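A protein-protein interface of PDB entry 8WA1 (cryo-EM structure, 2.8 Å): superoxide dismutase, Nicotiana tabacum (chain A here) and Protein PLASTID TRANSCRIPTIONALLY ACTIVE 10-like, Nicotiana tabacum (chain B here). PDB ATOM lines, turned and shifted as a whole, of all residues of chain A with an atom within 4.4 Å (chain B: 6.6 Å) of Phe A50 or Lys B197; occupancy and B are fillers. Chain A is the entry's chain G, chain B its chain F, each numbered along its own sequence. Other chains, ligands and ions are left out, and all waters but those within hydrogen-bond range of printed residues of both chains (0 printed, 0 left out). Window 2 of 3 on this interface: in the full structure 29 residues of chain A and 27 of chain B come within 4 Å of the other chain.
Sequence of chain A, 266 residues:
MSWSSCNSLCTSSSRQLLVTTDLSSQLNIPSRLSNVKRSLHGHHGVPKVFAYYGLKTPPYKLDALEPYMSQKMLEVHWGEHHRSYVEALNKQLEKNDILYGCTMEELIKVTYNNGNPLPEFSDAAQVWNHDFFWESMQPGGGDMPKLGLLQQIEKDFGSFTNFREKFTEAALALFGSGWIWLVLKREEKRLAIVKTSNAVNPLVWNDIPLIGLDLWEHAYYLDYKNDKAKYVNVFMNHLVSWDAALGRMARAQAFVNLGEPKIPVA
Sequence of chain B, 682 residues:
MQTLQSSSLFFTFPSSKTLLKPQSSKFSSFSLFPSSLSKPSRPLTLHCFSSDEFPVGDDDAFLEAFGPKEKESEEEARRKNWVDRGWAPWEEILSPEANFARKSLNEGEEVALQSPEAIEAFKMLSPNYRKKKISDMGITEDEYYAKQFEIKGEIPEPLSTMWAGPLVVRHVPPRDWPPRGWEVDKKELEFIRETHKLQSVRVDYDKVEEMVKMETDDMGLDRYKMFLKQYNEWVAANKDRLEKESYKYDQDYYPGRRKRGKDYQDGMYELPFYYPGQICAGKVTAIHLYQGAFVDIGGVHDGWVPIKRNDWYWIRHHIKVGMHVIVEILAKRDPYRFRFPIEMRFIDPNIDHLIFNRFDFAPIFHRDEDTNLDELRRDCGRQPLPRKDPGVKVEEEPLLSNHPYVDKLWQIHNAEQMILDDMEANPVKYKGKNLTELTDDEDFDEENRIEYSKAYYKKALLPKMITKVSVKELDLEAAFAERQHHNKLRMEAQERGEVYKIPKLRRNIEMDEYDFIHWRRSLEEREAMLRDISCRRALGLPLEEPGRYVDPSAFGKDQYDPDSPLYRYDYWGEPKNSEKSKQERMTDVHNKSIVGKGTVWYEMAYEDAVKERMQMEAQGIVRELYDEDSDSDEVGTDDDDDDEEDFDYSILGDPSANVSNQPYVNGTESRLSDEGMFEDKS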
ATOM      1  N   VAL A  49     -26.910 -15.307   2.415  1.00  0.00           N
ATOM      2  CA  VAL A  49     -27.949 -14.414   2.891  1.00  0.00           C
ATOM      3  C   VAL A  49     -27.399 -13.018   3.021  1.00  0.00           C
ATOM      4  O   VAL A  49     -28.093 -12.034   2.787  1.00  0.00           O
ATOM      5  CB  VAL A  49     -28.451 -14.843   4.269  1.00  0.00           C
ATOM      6  N   PHE A  50     -26.141 -12.933   3.402  1.00  0.00           N
ATOM      7  CA  PHE A  50     -25.538 -11.641   3.556  1.00  0.00           C
ATOM      8  C   PHE A  50     -24.550 -11.443   2.452  1.00  0.00           C
ATOM      9  O   PHE A  50     -23.612 -12.220   2.304  1.00  0.00           O
ATOM     10  CB  PHE A  50     -24.822 -11.556   4.891  1.00  0.00           C
ATOM     11  N   ALA A  51     -24.753 -10.399   1.676  1.00  0.00           N
ATOM     12  CA  ALA A  51     -23.835 -10.097   0.609  1.00  0.00           C
ATOM     13  C   ALA A  51     -23.685  -8.615   0.662  1.00  0.00           C
ATOM     14  O   ALA A  51     -24.566  -7.942   1.184  1.00  0.00           O
ATOM     15  CB  ALA A  51     -24.403 -10.535  -0.725  1.00  0.00           C
ATOM     16  N   TYR A  53     -22.070  -7.090   2.518  1.00  0.00           N
ATOM     17  CA  TYR A  53     -22.116  -6.732   3.914  1.00  0.00           C
ATOM     18  C   TYR A  53     -21.046  -5.752   4.297  1.00  0.00           C
ATOM     19  O   TYR A  53     -21.283  -4.850   5.093  1.00  0.00           O
ATOM     20  CB  TYR A  53     -22.020  -7.983   4.785  1.00  0.00           C
ATOM     21  N   GLY A  54     -19.865  -5.899   3.729  1.00  0.00           N
ATOM     22  CA  GLY A  54     -18.774  -5.073   4.184  1.00  0.00           C
ATOM     23  C   GLY A  54     -18.918  -3.590   4.091  1.00  0.00           C
ATOM     24  O   GLY A  54     -19.418  -3.054   3.110  1.00  0.00           O
ATOM     25  N   ASN A  90     -28.605  -6.393   2.880  1.00  0.00           N
ATOM     26  CA  ASN A  90     -28.478  -7.843   2.977  1.00  0.00           C
ATOM     27  C   ASN A  90     -29.755  -8.497   3.493  1.00  0.00           C
ATOM     28  O   ASN A  90     -30.068  -9.619   3.083  1.00  0.00           O
ATOM     29  CB  ASN A  90     -27.279  -8.248   3.849  1.00  0.00           C
ATOM     30  CG  ASN A  90     -27.171  -7.456   5.141  1.00  0.00           C
ATOM     31  OD1 ASN A  90     -26.137  -6.848   5.414  1.00  0.00           O
ATOM     32  ND2 ASN A  90     -28.219  -7.484   5.953  1.00  0.00           N
ATOM     33  N   TYR A 100     -30.628 -11.495  -5.310  1.00  0.00           N
ATOM     34  CA  TYR A 100     -29.428 -11.816  -4.545  1.00  0.00           C
ATOM     35  C   TYR A 100     -28.229 -12.038  -5.460  1.00  0.00           C
ATOM     36  O   TYR A 100     -27.147 -11.485  -5.226  1.00  0.00           O
ATOM     37  CB  TYR A 100     -29.682 -13.052  -3.681  1.00  0.00           C
ATOM     38  CG  TYR A 100     -28.584 -13.360  -2.688  1.00  0.00           C
ATOM     39  CD1 TYR A 100     -28.607 -12.819  -1.410  1.00  0.00           C
ATOM     40  CD2 TYR A 100     -27.532 -14.204  -3.022  1.00  0.00           C
ATOM     41  CE1 TYR A 100     -27.612 -13.101  -0.496  1.00  0.00           C
ATOM     42  CE2 TYR A 100     -26.531 -14.491  -2.115  1.00  0.00           C
ATOM     43  CZ  TYR A 100     -26.578 -13.940  -0.853  1.00  0.00           C
ATOM     44  OH  TYR A 100     -25.583 -14.221   0.054  1.00  0.00           O
ATOM     45  N   GLU B 190     -25.352 -20.938   3.545  1.00  0.00           N
ATOM     46  CA  GLU B 190     -24.877 -19.773   4.284  1.00  0.00           C
ATOM     47  C   GLU B 190     -23.357 -19.765   4.384  1.00  0.00           C
ATOM     48  O   GLU B 190     -22.719 -18.713   4.240  1.00  0.00           O
ATOM     49  CB  GLU B 190     -25.507 -19.741   5.678  1.00  0.00           C
ATOM     50  CG  GLU B 190     -27.024 -19.832   5.681  1.00  0.00           C
ATOM     51  CD  GLU B 190     -27.682 -18.729   4.875  1.00  0.00           C
ATOM     52  OE1 GLU B 190     -27.122 -17.614   4.822  1.00  0.00           O
ATOM     53  OE2 GLU B 190     -28.758 -18.977   4.291  1.00  0.00           O
ATOM     54  N   ARG B 193     -22.069 -18.654   1.045  1.00  0.00           N
ATOM     55  CA  ARG B 193     -22.302 -17.241   0.777  1.00  0.00           C
ATOM     56  C   ARG B 193     -21.554 -16.316   1.729  1.00  0.00           C
ATOM     57  O   ARG B 193     -21.498 -15.109   1.471  1.00  0.00           O
ATOM     58  CB  ARG B 193     -23.803 -16.941   0.837  1.00  0.00           C
ATOM     59  CG  ARG B 193     -24.610 -17.581  -0.286  1.00  0.00           C
ATOM     60  CD  ARG B 193     -26.104 -17.388  -0.083  1.00  0.00           C
ATOM     61  NE  ARG B 193     -26.877 -17.797  -1.254  1.00  0.00           N
ATOM     62  CZ  ARG B 193     -28.194 -17.657  -1.364  1.00  0.00           C
ATOM     63  NH1 ARG B 193     -28.890 -17.118  -0.372  1.00  0.00           N
ATOM     64  NH2 ARG B 193     -28.817 -18.055  -2.466  1.00  0.00           N
ATOM     65  N   GLU B 194     -20.984 -16.844   2.814  1.00  0.00           N
ATOM     66  CA  GLU B 194     -20.212 -16.015   3.733  1.00  0.00           C
ATOM     67  C   GLU B 194     -18.990 -15.378   3.078  1.00  0.00           C
ATOM     68  O   GLU B 194     -18.491 -14.369   3.587  1.00  0.00           O
ATOM     69  CB  GLU B 194     -19.778 -16.843   4.946  1.00  0.00           C
ATOM     70  CG  GLU B 194     -19.281 -16.022   6.128  1.00  0.00           C
ATOM     71  CD  GLU B 194     -18.875 -16.881   7.309  1.00  0.00           C
ATOM     72  OE1 GLU B 194     -19.032 -18.117   7.226  1.00  0.00           O
ATOM     73  OE2 GLU B 194     -18.396 -16.319   8.316  1.00  0.00           O
ATOM     74  N   THR B 195     -18.501 -15.932   1.966  1.00  0.00           N
ATOM     75  CA  THR B 195     -17.342 -15.348   1.296  1.00  0.00           C
ATOM     76  C   THR B 195     -17.686 -14.005   0.662  1.00  0.00           C
ATOM     77  O   THR B 195     -16.797 -13.187   0.395  1.00  0.00           O
ATOM     78  CB  THR B 195     -16.807 -16.313   0.236  1.00  0.00           C
ATOM     79  OG1 THR B 195     -16.818 -17.648   0.755  1.00  0.00           O
ATOM     80  CG2 THR B 195     -15.381 -15.947  -0.150  1.00  0.00           C
ATOM     81  N   HIS B 196     -18.974 -13.762   0.404  1.00  0.00           N
ATOM     82  CA  HIS B 196     -19.380 -12.510  -0.226  1.00  0.00           C
ATOM     83  C   HIS B 196     -19.078 -11.315   0.671  1.00  0.00           C
ATOM     84  O   HIS B 196     -18.636 -10.264   0.190  1.00  0.00           O
ATOM     85  CB  HIS B 196     -20.867 -12.564  -0.575  1.00  0.00           C
ATOM     86  CG  HIS B 196     -21.239 -13.736  -1.429  1.00  0.00           C
ATOM     87  ND1 HIS B 196     -20.327 -14.396  -2.224  1.00  0.00           N
ATOM     88  CD2 HIS B 196     -22.422 -14.371  -1.605  1.00  0.00           C
ATOM     89  CE1 HIS B 196     -20.933 -15.385  -2.858  1.00  0.00           C
ATOM     90  NE2 HIS B 196     -22.205 -15.391  -2.500  1.00  0.00           N
ATOM     91  N   LYS B 197     -19.308 -11.456   1.978  1.00  0.00           N
ATOM     92  CA  LYS B 197     -18.998 -10.366   2.897  1.00  0.00           C
ATOM     93  C   LYS B 197     -17.495 -10.253   3.129  1.00  0.00           C
ATOM     94  O   LYS B 197     -16.982  -9.161   3.403  1.00  0.00           O
ATOM     95  CB  LYS B 197     -19.738 -10.564   4.222  1.00  0.00           C
ATOM     96  CG  LYS B 197     -19.221 -11.711   5.073  1.00  0.00           C
ATOM     97  CD  LYS B 197     -20.074 -11.913   6.314  1.00  0.00           C
ATOM     98  CE  LYS B 197     -21.472 -12.385   5.953  1.00  0.00           C
ATOM     99  NZ  LYS B 197     -22.280 -12.683   7.166  1.00  0.00           N
ATOM    100  N   LEU B 198     -16.772 -11.371   3.023  1.00  0.00           N
ATOM    101  CA  LEU B 198     -15.326 -11.343   3.213  1.00  0.00           C
ATOM    102  C   LEU B 198     -14.601 -10.736   2.020  1.00  0.00           C
ATOM    103  O   LEU B 198     -13.498 -10.203   2.184  1.00  0.00           O
ATOM    104  CB  LEU B 198     -14.800 -12.755   3.478  1.00  0.00           C
ATOM    105  CG  LEU B 198     -15.369 -13.473   4.705  1.00  0.00           C
ATOM    106  CD1 LEU B 198     -14.710 -14.831   4.884  1.00  0.00           C
ATOM    107  CD2 LEU B 198     -15.199 -12.620   5.952  1.00  0.00           C
ATOM    108  N   GLN B 199     -15.191 -10.809   0.828  1.00  0.00           N
ATOM    109  CA  GLN B 199     -14.575 -10.256  -0.372  1.00  0.00           C
ATOM    110  C   GLN B 199     -14.463  -8.733  -0.342  1.00  0.00           C
ATOM    111  O   GLN B 199     -13.784  -8.161  -1.203  1.00  0.00           O
ATOM    112  CB  GLN B 199     -15.370 -10.699  -1.604  1.00  0.00           C
ATOM    113  CG  GLN B 199     -14.636 -10.552  -2.929  1.00  0.00           C
ATOM    114  CD  GLN B 199     -15.491 -10.960  -4.112  1.00  0.00           C
ATOM    115  OE1 GLN B 199     -16.674 -11.265  -3.964  1.00  0.00           O
ATOM    116  NE2 GLN B 199     -14.893 -10.967  -5.298  1.00  0.00           N
ATOM    117  N   SER B 200     -15.082  -8.067   0.634  1.00  0.00           N
ATOM    118  CA  SER B 200     -15.080  -6.613   0.726  1.00  0.00           C
ATOM    119  C   SER B 200     -14.020  -6.091   1.691  1.00  0.00           C
ATOM    120  O   SER B 200     -14.245  -5.085   2.374  1.00  0.00           O
ATOM    121  CB  SER B 200     -16.465  -6.111   1.133  1.00  0.00           C
ATOM    122  OG  SER B 200     -16.909  -6.746   2.320  1.00  0.00           O
ATOM    123  N   VAL B 201     -12.871  -6.758   1.768  1.00  0.00           N
ATOM    124  CA  VAL B 201     -11.760  -6.341   2.618  1.00  0.00           C
ATOM    125  C   VAL B 201     -10.618  -5.896   1.714  1.00  0.00           C
ATOM    126  O   VAL B 201     -10.205  -6.637   0.814  1.00  0.00           O
ATOM    127  CB  VAL B 201     -11.311  -7.469   3.559  1.00  0.00           C
ATOM    128  CG1 VAL B 201     -10.154  -7.002   4.432  1.00  0.00           C
ATOM    129  CG2 VAL B 201     -12.478  -7.941   4.412  1.00  0.00           C
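Val A49 touches Arg B193.
Phe A50 touches Arg B193.
His B196 touches Phe A50.
CB of Phe A50 touches NZ of Lys B197, 3.6 Å away.
Lys B197 touches Tyr A53 (CB to CB, 3.5 Å).
CD of Arg B193 touches OH of Tyr A100, 3.2 Å away.
His B196 touches Tyr A100 (CD2 to OH, 3.6 Å).
Asn A90 touches none of the printed residues of chain B.
Printed residues of chain B within 4 Å of Tyr A100: Arg B193 (3.2 Å) and His B196 (3.6 Å).
Glu B194 touches none of the printed residues of chain A.
Lys B197 touches just these residues of chain A: Phe A50 (3.6 Å) and Tyr A53 (3.5 Å).
Of the printed residues of chain A, Ser B200 touches Gly A54.
The nearest printed residue of chain B that does not touch Phe A50 is Glu B190 (5.0 Å).
The backbone NH of Val A49 sits close to the side-chain carboxylate of Glu B190 (3.3 Å).
The backbone NH (N) of Gly A54 lies close to the side-chain hydroxyl (OG) of Ser B200 (3.4 Å).
Printed residues of chain B that touch a printed residue of chain A: Glu B190, Arg B193, His B196, Lys B197 and Ser B200.
Hydrophobic or aromatic side chains of chain B within 4 Å of the printed part of chain A: His B196.
Among the printed residues, no Asp or Glu carboxylate lies within 4 Å of a Lys or Arg side-chain nitrogen of the other chain.
O of Lys B197 lies within hydrogen-bond range of OG of Ser B200 (2.6 Å).
The side-chain hydroxyl of Tyr A100 is in hydrogen-bond range of the backbone NH of Val A49.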
